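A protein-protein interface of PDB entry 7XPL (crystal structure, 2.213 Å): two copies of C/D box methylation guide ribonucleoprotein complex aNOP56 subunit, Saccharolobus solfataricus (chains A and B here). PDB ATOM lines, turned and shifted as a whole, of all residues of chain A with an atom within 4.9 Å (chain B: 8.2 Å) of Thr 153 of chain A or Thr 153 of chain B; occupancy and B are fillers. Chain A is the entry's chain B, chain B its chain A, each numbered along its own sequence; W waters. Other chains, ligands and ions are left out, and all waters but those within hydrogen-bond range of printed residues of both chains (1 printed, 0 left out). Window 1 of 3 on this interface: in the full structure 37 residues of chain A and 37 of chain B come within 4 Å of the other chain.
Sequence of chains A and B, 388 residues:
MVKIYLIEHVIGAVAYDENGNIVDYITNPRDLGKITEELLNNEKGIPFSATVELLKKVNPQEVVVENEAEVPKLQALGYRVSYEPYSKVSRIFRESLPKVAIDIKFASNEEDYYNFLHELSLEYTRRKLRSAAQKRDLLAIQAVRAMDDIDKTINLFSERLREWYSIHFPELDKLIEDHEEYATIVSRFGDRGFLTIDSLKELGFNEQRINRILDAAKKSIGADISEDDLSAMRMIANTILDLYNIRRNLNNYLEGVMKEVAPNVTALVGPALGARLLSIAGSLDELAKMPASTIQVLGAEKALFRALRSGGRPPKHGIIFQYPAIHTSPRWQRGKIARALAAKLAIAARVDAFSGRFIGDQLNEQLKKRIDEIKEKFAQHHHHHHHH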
ATOM      1  N   ASP A 149     -24.110  24.023   7.360  1.00  0.00           N
ATOM      2  CA  ASP A 149     -23.143  24.326   8.405  1.00  0.00           C
ATOM      3  C   ASP A 149     -23.810  24.479   9.766  1.00  0.00           C
ATOM      4  O   ASP A 149     -23.302  23.987  10.771  1.00  0.00           O
ATOM      5  CB  ASP A 149     -22.384  25.614   8.073  1.00  0.00           C
ATOM      6  CG  ASP A 149     -21.653  25.540   6.753  1.00  0.00           C
ATOM      7  OD1 ASP A 149     -21.311  24.424   6.327  1.00  0.00           O
ATOM      8  OD2 ASP A 149     -21.419  26.612   6.137  1.00  0.00           O
ATOM      9  N   ILE A 150     -24.936  25.184   9.825  1.00  0.00           N
ATOM     10  CA  ILE A 150     -25.585  25.431  11.109  1.00  0.00           C
ATOM     11  C   ILE A 150     -26.132  24.133  11.708  1.00  0.00           C
ATOM     12  O   ILE A 150     -25.929  23.855  12.895  1.00  0.00           O
ATOM     13  CB  ILE A 150     -26.667  26.510  10.939  1.00  0.00           C
ATOM     14  CG1 ILE A 150     -25.963  27.838  10.662  1.00  0.00           C
ATOM     15  CG2 ILE A 150     -27.605  26.594  12.157  1.00  0.00           C
ATOM     16  CD1 ILE A 150     -26.848  29.028  10.769  1.00  0.00           C
ATOM     17  N   ASP A 151     -26.799  23.311  10.899  1.00  0.00           N
ATOM     18  CA  ASP A 151     -27.290  22.020  11.381  1.00  0.00           C
ATOM     19  C   ASP A 151     -26.162  21.179  11.967  1.00  0.00           C
ATOM     20  O   ASP A 151     -26.289  20.601  13.053  1.00  0.00           O
ATOM     21  CB  ASP A 151     -27.965  21.249  10.242  1.00  0.00           C
ATOM     22  CG  ASP A 151     -29.365  21.788   9.909  1.00  0.00           C
ATOM     23  OD1 ASP A 151     -29.913  22.567  10.728  1.00  0.00           O
ATOM     24  OD2 ASP A 151     -29.926  21.425   8.833  1.00  0.00           O
ATOM     25  N   LYS A 152     -25.072  21.053  11.220  1.00  0.00           N
ATOM     26  CA  LYS A 152     -23.920  20.295  11.681  1.00  0.00           C
ATOM     27  C   LYS A 152     -23.368  20.859  12.992  1.00  0.00           C
ATOM     28  O   LYS A 152     -23.023  20.107  13.908  1.00  0.00           O
ATOM     29  CB  LYS A 152     -22.873  20.329  10.577  1.00  0.00           C
ATOM     30  CG  LYS A 152     -21.523  19.780  10.902  1.00  0.00           C
ATOM     31  CD  LYS A 152     -20.769  19.769   9.576  1.00  0.00           C
ATOM     32  CE  LYS A 152     -19.363  19.263   9.715  1.00  0.00           C
ATOM     33  NZ  LYS A 152     -18.874  18.980   8.322  1.00  0.00           N
ATOM     34  N   THR A 153     -23.278  22.179  13.090  1.00  0.00           N
ATOM     35  CA  THR A 153     -22.829  22.831  14.305  1.00  0.00           C
ATOM     36  C   THR A 153     -23.795  22.584  15.452  1.00  0.00           C
ATOM     37  O   THR A 153     -23.369  22.336  16.586  1.00  0.00           O
ATOM     38  CB  THR A 153     -22.678  24.323  14.039  1.00  0.00           C
ATOM     39  OG1 THR A 153     -21.805  24.501  12.928  1.00  0.00           O
ATOM     40  CG2 THR A 153     -22.128  25.057  15.223  1.00  0.00           C
ATOM     41  N   ILE A 154     -25.096  22.669  15.187  1.00  0.00           N
ATOM     42  CA  ILE A 154     -26.058  22.423  16.250  1.00  0.00           C
ATOM     43  C   ILE A 154     -25.844  21.035  16.814  1.00  0.00           C
ATOM     44  O   ILE A 154     -25.868  20.828  18.031  1.00  0.00           O
ATOM     45  CB  ILE A 154     -27.490  22.588  15.723  1.00  0.00           C
ATOM     46  CG1 ILE A 154     -27.792  24.063  15.450  1.00  0.00           C
ATOM     47  CG2 ILE A 154     -28.491  21.958  16.685  1.00  0.00           C
ATOM     48  CD1 ILE A 154     -29.241  24.270  14.986  1.00  0.00           C
ATOM     49  N   ASN A 155     -25.611  20.070  15.932  1.00  0.00           N
ATOM     50  CA  ASN A 155     -25.433  18.705  16.375  1.00  0.00           C
ATOM     51  C   ASN A 155     -24.096  18.532  17.106  1.00  0.00           C
ATOM     52  O   ASN A 155     -24.046  17.923  18.171  1.00  0.00           O
ATOM     53  CB  ASN A 155     -25.548  17.783  15.175  1.00  0.00           C
ATOM     54  CG  ASN A 155     -25.469  16.338  15.560  1.00  0.00           C
ATOM     55  OD1 ASN A 155     -26.166  15.899  16.480  1.00  0.00           O
ATOM     56  ND2 ASN A 155     -24.608  15.580  14.872  1.00  0.00           N
ATOM     57  N   LEU A 156     -23.024  19.116  16.570  1.00  0.00           N
ATOM     58  CA  LEU A 156     -21.721  19.064  17.218  1.00  0.00           C
ATOM     59  C   LEU A 156     -21.782  19.615  18.640  1.00  0.00           C
ATOM     60  O   LEU A 156     -21.371  18.941  19.585  1.00  0.00           O
ATOM     61  CB  LEU A 156     -20.688  19.836  16.387  1.00  0.00           C
ATOM     62  CG  LEU A 156     -19.304  19.935  17.037  1.00  0.00           C
ATOM     63  CD1 LEU A 156     -18.722  18.533  17.222  1.00  0.00           C
ATOM     64  CD2 LEU A 156     -18.355  20.788  16.207  1.00  0.00           C
ATOM     65  N   PHE A 157     -22.319  20.835  18.807  1.00  0.00           N
ATOM     66  CA  PHE A 157     -22.365  21.487  20.117  1.00  0.00           C
ATOM     67  C   PHE A 157     -23.330  20.789  21.064  1.00  0.00           C
ATOM     68  O   PHE A 157     -23.121  20.806  22.284  1.00  0.00           O
ATOM     69  CB  PHE A 157     -22.818  22.949  19.987  1.00  0.00           C
ATOM     70  CG  PHE A 157     -21.820  23.873  19.333  1.00  0.00           C
ATOM     71  CD1 PHE A 157     -20.687  23.392  18.730  1.00  0.00           C
ATOM     72  CD2 PHE A 157     -22.053  25.244  19.312  1.00  0.00           C
ATOM     73  CE1 PHE A 157     -19.780  24.272  18.112  1.00  0.00           C
ATOM     74  CE2 PHE A 157     -21.166  26.140  18.690  1.00  0.00           C
ATOM     75  CZ  PHE A 157     -20.020  25.654  18.099  1.00  0.00           C
ATOM     76  N   SER A 158     -24.425  20.244  20.535  1.00  0.00           N
ATOM     77  CA  SER A 158     -25.357  19.507  21.371  1.00  0.00           C
ATOM     78  C   SER A 158     -24.733  18.217  21.866  1.00  0.00           C
ATOM     79  O   SER A 158     -25.049  17.761  22.972  1.00  0.00           O
ATOM     80  CB  SER A 158     -26.651  19.185  20.611  1.00  0.00           C
ATOM     81  OG  SER A 158     -27.351  20.373  20.283  1.00  0.00           O
ATOM     82  N   LEU A 243     -28.622  29.241  17.613  1.00  0.00           N
ATOM     83  CA  LEU A 243     -28.378  28.652  16.299  1.00  0.00           C
ATOM     84  C   LEU A 243     -29.664  28.115  15.691  1.00  0.00           C
ATOM     85  O   LEU A 243     -29.867  28.199  14.477  1.00  0.00           O
ATOM     86  CB  LEU A 243     -27.326  27.544  16.396  1.00  0.00           C
ATOM     87  CG  LEU A 243     -25.868  27.985  16.532  1.00  0.00           C
ATOM     88  CD1 LEU A 243     -24.967  26.744  16.673  1.00  0.00           C
ATOM     89  CD2 LEU A 243     -25.479  28.791  15.319  1.00  0.00           C
ATOM     90  N   ALA B 146     -15.014  21.902  23.881  1.00  0.00           N
ATOM     91  CA  ALA B 146     -15.993  22.837  23.340  1.00  0.00           C
ATOM     92  C   ALA B 146     -15.295  24.037  22.710  1.00  0.00           C
ATOM     93  O   ALA B 146     -15.779  24.579  21.718  1.00  0.00           O
ATOM     94  CB  ALA B 146     -16.980  23.280  24.420  1.00  0.00           C
ATOM     95  N   MET B 147     -14.134  24.427  23.236  1.00  0.00           N
ATOM     96  CA  MET B 147     -13.405  25.541  22.653  1.00  0.00           C
ATOM     97  C   MET B 147     -12.887  25.176  21.274  1.00  0.00           C
ATOM     98  O   MET B 147     -12.856  26.017  20.364  1.00  0.00           O
ATOM     99  CB  MET B 147     -12.248  25.950  23.567  1.00  0.00           C
ATOM    100  CG  MET B 147     -11.859  27.415  23.406  1.00  0.00           C
ATOM    101  SD  MET B 147     -10.593  27.988  24.548  1.00  0.00           S
ATOM    102  CE  MET B 147      -9.168  27.111  23.917  1.00  0.00           C
ATOM    103  N   ASP B 148     -12.482  23.921  21.095  1.00  0.00           N
ATOM    104  CA  ASP B 148     -11.991  23.510  19.791  1.00  0.00           C
ATOM    105  C   ASP B 148     -13.151  23.382  18.786  1.00  0.00           C
ATOM    106  O   ASP B 148     -12.979  23.682  17.601  1.00  0.00           O
ATOM    107  CB  ASP B 148     -11.196  22.208  19.933  1.00  0.00           C
ATOM    108  CG  ASP B 148      -9.827  22.420  20.618  1.00  0.00           C
ATOM    109  OD1 ASP B 148      -9.352  23.588  20.678  1.00  0.00           O
ATOM    110  OD2 ASP B 148      -9.222  21.418  21.081  1.00  0.00           O
ATOM    111  N   ASP B 149     -14.334  22.962  19.234  1.00  0.00           N
ATOM    112  CA  ASP B 149     -15.500  23.009  18.353  1.00  0.00           C
ATOM    113  C   ASP B 149     -15.776  24.443  17.918  1.00  0.00           C
ATOM    114  O   ASP B 149     -15.954  24.728  16.724  1.00  0.00           O
ATOM    115  CB  ASP B 149     -16.721  22.423  19.056  1.00  0.00           C
ATOM    116  CG  ASP B 149     -16.527  20.959  19.441  1.00  0.00           C
ATOM    117  OD1 ASP B 149     -15.758  20.243  18.728  1.00  0.00           O
ATOM    118  OD2 ASP B 149     -17.139  20.549  20.462  1.00  0.00           O
ATOM    119  N   ILE B 150     -15.753  25.363  18.887  1.00  0.00           N
ATOM    120  CA  ILE B 150     -15.965  26.776  18.622  1.00  0.00           C
ATOM    121  C   ILE B 150     -14.958  27.296  17.599  1.00  0.00           C
ATOM    122  O   ILE B 150     -15.328  27.963  16.623  1.00  0.00           O
ATOM    123  CB  ILE B 150     -15.927  27.559  19.944  1.00  0.00           C
ATOM    124  CG1 ILE B 150     -17.239  27.283  20.685  1.00  0.00           C
ATOM    125  CG2 ILE B 150     -15.715  29.046  19.676  1.00  0.00           C
ATOM    126  CD1 ILE B 150     -17.273  27.799  22.071  1.00  0.00           C
ATOM    127  N   ASP B 151     -13.684  26.974  17.778  1.00  0.00           N
ATOM    128  CA  ASP B 151     -12.673  27.399  16.806  1.00  0.00           C
ATOM    129  C   ASP B 151     -12.982  26.868  15.415  1.00  0.00           C
ATOM    130  O   ASP B 151     -12.936  27.609  14.426  1.00  0.00           O
ATOM    131  CB  ASP B 151     -11.285  26.921  17.230  1.00  0.00           C
ATOM    132  CG  ASP B 151     -10.726  27.713  18.381  1.00  0.00           C
ATOM    133  OD1 ASP B 151     -11.308  28.792  18.668  1.00  0.00           O
ATOM    134  OD2 ASP B 151      -9.697  27.256  18.986  1.00  0.00           O
ATOM    135  N   LYS B 152     -13.239  25.565  15.324  1.00  0.00           N
ATOM    136  CA  LYS B 152     -13.610  24.938  14.063  1.00  0.00           C
ATOM    137  C   LYS B 152     -14.828  25.623  13.444  1.00  0.00           C
ATOM    138  O   LYS B 152     -14.860  25.871  12.237  1.00  0.00           O
ATOM    139  CB  LYS B 152     -13.884  23.455  14.320  1.00  0.00           C
ATOM    140  CG  LYS B 152     -14.322  22.587  13.138  1.00  0.00           C
ATOM    141  CD  LYS B 152     -14.102  21.094  13.531  1.00  0.00           C
ATOM    142  CE  LYS B 152     -14.470  20.130  12.376  1.00  0.00           C
ATOM    143  NZ  LYS B 152     -14.156  18.661  12.719  1.00  0.00           N
ATOM    144  N   THR B 153     -15.838  25.921  14.265  1.00  0.00           N
ATOM    145  CA  THR B 153     -17.065  26.538  13.794  1.00  0.00           C
ATOM    146  C   THR B 153     -16.817  27.954  13.312  1.00  0.00           C
ATOM    147  O   THR B 153     -17.270  28.336  12.226  1.00  0.00           O
ATOM    148  CB  THR B 153     -18.100  26.548  14.909  1.00  0.00           C
ATOM    149  OG1 THR B 153     -18.321  25.210  15.333  1.00  0.00           O
ATOM    150  CG2 THR B 153     -19.421  27.146  14.409  1.00  0.00           C
ATOM    151  N   ILE B 154     -16.103  28.751  14.114  1.00  0.00           N
ATOM    152  CA  ILE B 154     -15.764  30.108  13.698  1.00  0.00           C
ATOM    153  C   ILE B 154     -15.126  30.083  12.320  1.00  0.00           C
ATOM    154  O   ILE B 154     -15.475  30.880  11.432  1.00  0.00           O
ATOM    155  CB  ILE B 154     -14.843  30.772  14.737  1.00  0.00           C
ATOM    156  CG1 ILE B 154     -15.661  31.178  15.962  1.00  0.00           C
ATOM    157  CG2 ILE B 154     -14.086  31.986  14.138  1.00  0.00           C
ATOM    158  CD1 ILE B 154     -14.829  31.712  17.099  1.00  0.00           C
ATOM    159  N   ASN B 155     -14.211  29.144  12.103  1.00  0.00           N
ATOM    160  CA  ASN B 155     -13.535  29.105  10.818  1.00  0.00           C
ATOM    161  C   ASN B 155     -14.491  28.686   9.709  1.00  0.00           C
ATOM    162  O   ASN B 155     -14.443  29.245   8.609  1.00  0.00           O
ATOM    163  CB  ASN B 155     -12.347  28.163  10.868  1.00  0.00           C
ATOM    164  CG  ASN B 155     -11.546  28.199   9.603  1.00  0.00           C
ATOM    165  OD1 ASN B 155     -11.206  29.269   9.099  1.00  0.00           O
ATOM    166  ND2 ASN B 155     -11.227  27.036   9.077  1.00  0.00           N
ATOM    167  N   LEU B 156     -15.360  27.705   9.980  1.00  0.00           N
ATOM    168  CA  LEU B 156     -16.280  27.222   8.959  1.00  0.00           C
ATOM    169  C   LEU B 156     -17.269  28.317   8.544  1.00  0.00           C
ATOM    170  O   LEU B 156     -17.494  28.539   7.357  1.00  0.00           O
ATOM    171  CB  LEU B 156     -17.013  25.968   9.467  1.00  0.00           C
ATOM    172  CG  LEU B 156     -18.256  25.495   8.688  1.00  0.00           C
ATOM    173  CD1 LEU B 156     -17.921  25.076   7.246  1.00  0.00           C
ATOM    174  CD2 LEU B 156     -18.963  24.364   9.429  1.00  0.00           C
ATOM    175  N   PHE B 157     -17.848  29.026   9.516  1.00  0.00           N
ATOM    176  CA  PHE B 157     -18.810  30.080   9.199  1.00  0.00           C
ATOM    177  C   PHE B 157     -18.127  31.245   8.490  1.00  0.00           C
ATOM    178  O   PHE B 157     -18.714  31.864   7.585  1.00  0.00           O
ATOM    179  CB  PHE B 157     -19.485  30.589  10.480  1.00  0.00           C
ATOM    180  CG  PHE B 157     -20.446  29.628  11.130  1.00  0.00           C
ATOM    181  CD1 PHE B 157     -20.661  28.347  10.630  1.00  0.00           C
ATOM    182  CD2 PHE B 157     -21.155  30.030  12.263  1.00  0.00           C
ATOM    183  CE1 PHE B 157     -21.595  27.492  11.247  1.00  0.00           C
ATOM    184  CE2 PHE B 157     -22.069  29.182  12.900  1.00  0.00           C
ATOM    185  CZ  PHE B 157     -22.308  27.916  12.377  1.00  0.00           C
ATOM    186  N   SER B 158     -16.895  31.584   8.918  1.00  0.00           N
ATOM    187  CA  SER B 158     -16.180  32.705   8.317  1.00  0.00           C
ATOM    188  C   SER B 158     -15.848  32.412   6.865  1.00  0.00           C
ATOM    189  O   SER B 158     -15.930  33.301   6.006  1.00  0.00           O
ATOM    190  CB  SER B 158     -14.886  33.011   9.093  1.00  0.00           C
ATOM    191  OG  SER B 158     -15.136  33.395  10.444  1.00  0.00           O
ATOM    192  N   GLU B 159     -15.455  31.168   6.577  1.00  0.00           N
ATOM    193  CA  GLU B 159     -15.206  30.783   5.197  1.00  0.00           C
ATOM    194  C   GLU B 159     -16.484  30.881   4.371  1.00  0.00           C
ATOM    195  O   GLU B 159     -16.435  31.255   3.197  1.00  0.00           O
ATOM    196  CB  GLU B 159     -14.645  29.370   5.139  1.00  0.00           C
ATOM    197  CG  GLU B 159     -13.243  29.263   5.747  1.00  0.00           C
ATOM    198  CD  GLU B 159     -12.195  28.985   4.693  1.00  0.00           C
ATOM    199  OE1 GLU B 159     -11.551  27.899   4.787  1.00  0.00           O
ATOM    200  OE2 GLU B 159     -12.031  29.845   3.778  1.00  0.00           O
ATOM    201  N   ARG B 160     -17.633  30.544   4.980  1.00  0.00           N
ATOM    202  CA  ARG B 160     -18.900  30.588   4.267  1.00  0.00           C
ATOM    203  C   ARG B 160     -19.355  32.028   4.079  1.00  0.00           C
ATOM    204  O   ARG B 160     -19.810  32.393   2.994  1.00  0.00           O
ATOM    205  CB  ARG B 160     -19.972  29.792   5.007  1.00  0.00           C
ATOM    206  CG  ARG B 160     -21.324  29.714   4.186  1.00  0.00           C
ATOM    207  CD  ARG B 160     -21.237  28.684   3.013  1.00  0.00           C
ATOM    208  NE  ARG B 160     -20.833  27.374   3.526  1.00  0.00           N
ATOM    209  CZ  ARG B 160     -20.197  26.421   2.839  1.00  0.00           C
ATOM    210  NH1 ARG B 160     -19.859  25.278   3.450  1.00  0.00           N
ATOM    211  NH2 ARG B 160     -19.870  26.615   1.569  1.00  0.00           N
ATOM    212  N   HIS B 179     -10.857  37.357  10.286  1.00  0.00           N
ATOM    213  CA  HIS B 179     -12.261  36.976  10.213  1.00  0.00           C
ATOM    214  C   HIS B 179     -13.126  37.832  11.118  1.00  0.00           C
ATOM    215  O   HIS B 179     -14.274  38.146  10.769  1.00  0.00           O
ATOM    216  CB  HIS B 179     -12.461  35.507  10.579  1.00  0.00           C
ATOM    217  CG  HIS B 179     -11.805  34.557   9.634  1.00  0.00           C
ATOM    218  ND1 HIS B 179     -11.526  34.887   8.325  1.00  0.00           N
ATOM    219  CD2 HIS B 179     -11.311  33.308   9.824  1.00  0.00           C
ATOM    220  CE1 HIS B 179     -10.914  33.876   7.738  1.00  0.00           C
ATOM    221  NE2 HIS B 179     -10.775  32.904   8.625  1.00  0.00           N
ATOM    222  N   ILE B 236     -25.195  35.268   9.768  1.00  0.00           N
ATOM    223  CA  ILE B 236     -23.960  34.518   9.964  1.00  0.00           C
ATOM    224  C   ILE B 236     -22.892  35.418  10.572  1.00  0.00           C
ATOM    225  O   ILE B 236     -22.130  34.990  11.444  1.00  0.00           O
ATOM    226  CB  ILE B 236     -23.496  33.898   8.636  1.00  0.00           C
ATOM    227  CG1 ILE B 236     -24.631  33.131   7.971  1.00  0.00           C
ATOM    228  CG2 ILE B 236     -22.322  32.974   8.860  1.00  0.00           C
ATOM    229  CD1 ILE B 236     -25.371  32.193   8.899  1.00  0.00           C
ATOM    230  N   THR B 239     -23.484  35.835  14.368  1.00  0.00           N
ATOM    231  CA  THR B 239     -23.127  34.585  15.023  1.00  0.00           C
ATOM    232  C   THR B 239     -21.616  34.441  15.156  1.00  0.00           C
ATOM    233  O   THR B 239     -21.116  33.995  16.194  1.00  0.00           O
ATOM    234  CB  THR B 239     -23.692  33.396  14.250  1.00  0.00           C
ATOM    235  OG1 THR B 239     -25.105  33.536  14.167  1.00  0.00           O
ATOM    236  CG2 THR B 239     -23.364  32.061  14.952  1.00  0.00           C
ATOM    237  N   ILE B 240     -20.870  34.787  14.109  1.00  0.00           N
ATOM    238  CA  ILE B 240     -19.423  34.722  14.218  1.00  0.00           C
ATOM    239  C   ILE B 240     -18.948  35.594  15.373  1.00  0.00           C
ATOM    240  O   ILE B 240     -18.124  35.170  16.200  1.00  0.00           O
ATOM    241  CB  ILE B 240     -18.764  35.123  12.889  1.00  0.00           C
ATOM    242  CG1 ILE B 240     -19.081  34.071  11.822  1.00  0.00           C
ATOM    243  CG2 ILE B 240     -17.254  35.295  13.068  1.00  0.00           C
ATOM    244  CD1 ILE B 240     -18.678  34.483  10.425  1.00  0.00           C
ATOM    245  N   LEU B 243     -19.625  34.083  18.653  1.00  0.00           N
ATOM    246  CA  LEU B 243     -18.777  32.927  18.904  1.00  0.00           C
ATOM    247  C   LEU B 243     -17.386  33.351  19.365  1.00  0.00           C
ATOM    248  O   LEU B 243     -16.797  32.693  20.225  1.00  0.00           O
ATOM    249  CB  LEU B 243     -18.698  32.045  17.655  1.00  0.00           C
ATOM    250  CG  LEU B 243     -19.909  31.158  17.393  1.00  0.00           C
ATOM    251  CD1 LEU B 243     -19.739  30.396  16.068  1.00  0.00           C
ATOM    252  CD2 LEU B 243     -20.148  30.186  18.524  1.00  0.00           C
HETATM  253  O   HOH W   1     -19.087  23.492  13.261  1.00  0.00           O
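The guanidinium group (NE) of Arg 160 of chain B lies within salt-bridge range of the side-chain carboxylate (OD2) of Asp 149 of chain A, at 2.8 Å.
The backbone carbonyl oxygen (O) of Asp 149 of chain B lies within hydrogen-bond range of the side-chain hydroxyl (OG1) of Thr 153 of chain B (2.8 Å).
The side-chain hydroxyl (OG1) of Thr 153 of chain A is in hydrogen-bond range of the backbone carbonyl oxygen (O) of Asp 149 of chain A, 2.7 Å away.
Asp 149 of chain A touches Leu 156 of chain B (OD1 to CD1, 3.6 Å).
Phe 157 of chain B touches Asp 149 of chain A (CE1 to CB, 3.8 Å).
Ile 150 of chain A touches Ile 236 of chain B.
Thr 153 of chain A touches Thr 153 of chain B (CG2 to CG2, 3.5 Å).
Phe 157 of chain B touches Thr 153 of chain A.
Asp 149 of chain B touches Leu 156 of chain A (OD1 to CD2, 3.7 Å).
Phe 157 of chain A touches Asp 149 of chain B.
Phe 157 of chain A touches Thr 153 of chain B (CE1 to OG1, 3.3 Å).
Leu 243 of chain A touches Thr 239 of chain B (CD2 to CG2, 3.9 Å).
Thr 153 of chain B touches just these residues of chain A: Thr 153 and Phe 157.
Of the printed residues of chain B, Leu 243 of chain A touches Thr 239.
Of the printed residues of chain B, Leu 156 of chain A touches Asp 149 (3.7 Å).
Of the printed residues of chain B, Ile 150 of chain A touches Ile 236 (3.96 Å).
Of the printed residues of chain A, Phe 157 of chain B touches Asp 149 and Thr 153.
Lys 152 of chain A touches none of the printed residues of chain B.
The nearest residue of chain A that does not touch Thr 153 of chain B is Leu 156 of chain A (4.5 Å).
The nearest printed residue of chain B that does not touch Leu 243 of chain A is Phe 157 of chain B (4.2 Å).
Printed residues of chain A that touch a printed residue of chain B: Asp 149, Ile 150, Thr 153, Leu 156, Phe 157 and Leu 243.
Hydrophobic or aromatic side chains of chain B within 4 Å of the printed part of chain A: Leu 156, Phe 157 and Ile 236.
Among the printed residues, Asp or Glu carboxylates within 4 Å of a Lys or Arg side-chain nitrogen of the other chain: Asp 149 of chain A with Arg 160 of chain B (2.8 Å).
Asp 149 of chain A touches Leu 156 of chain B, and with the chains exchanged Leu 156 of chain A touches Asp 149 of chain B.
Asp 149 of chain A touches Phe 157 of chain B, and with the chains exchanged Phe 157 of chain A touches Asp 149 of chain B.
Thr 153 of chain A touches its own counterpart, Thr 153 of chain B.
Thr 153 of chain A touches Phe 157 of chain B, and with the chains exchanged Phe 157 of chain A touches Thr 153 of chain B.
Of the 10 pairs that touch across the chains among the printed residues, 7 have their exchanged pair printed and touching as well.
Water W1 bridges the side-chain hydroxyl of Thr 153 of chain B and the side-chain hydroxyl of Thr 153 of chain A.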
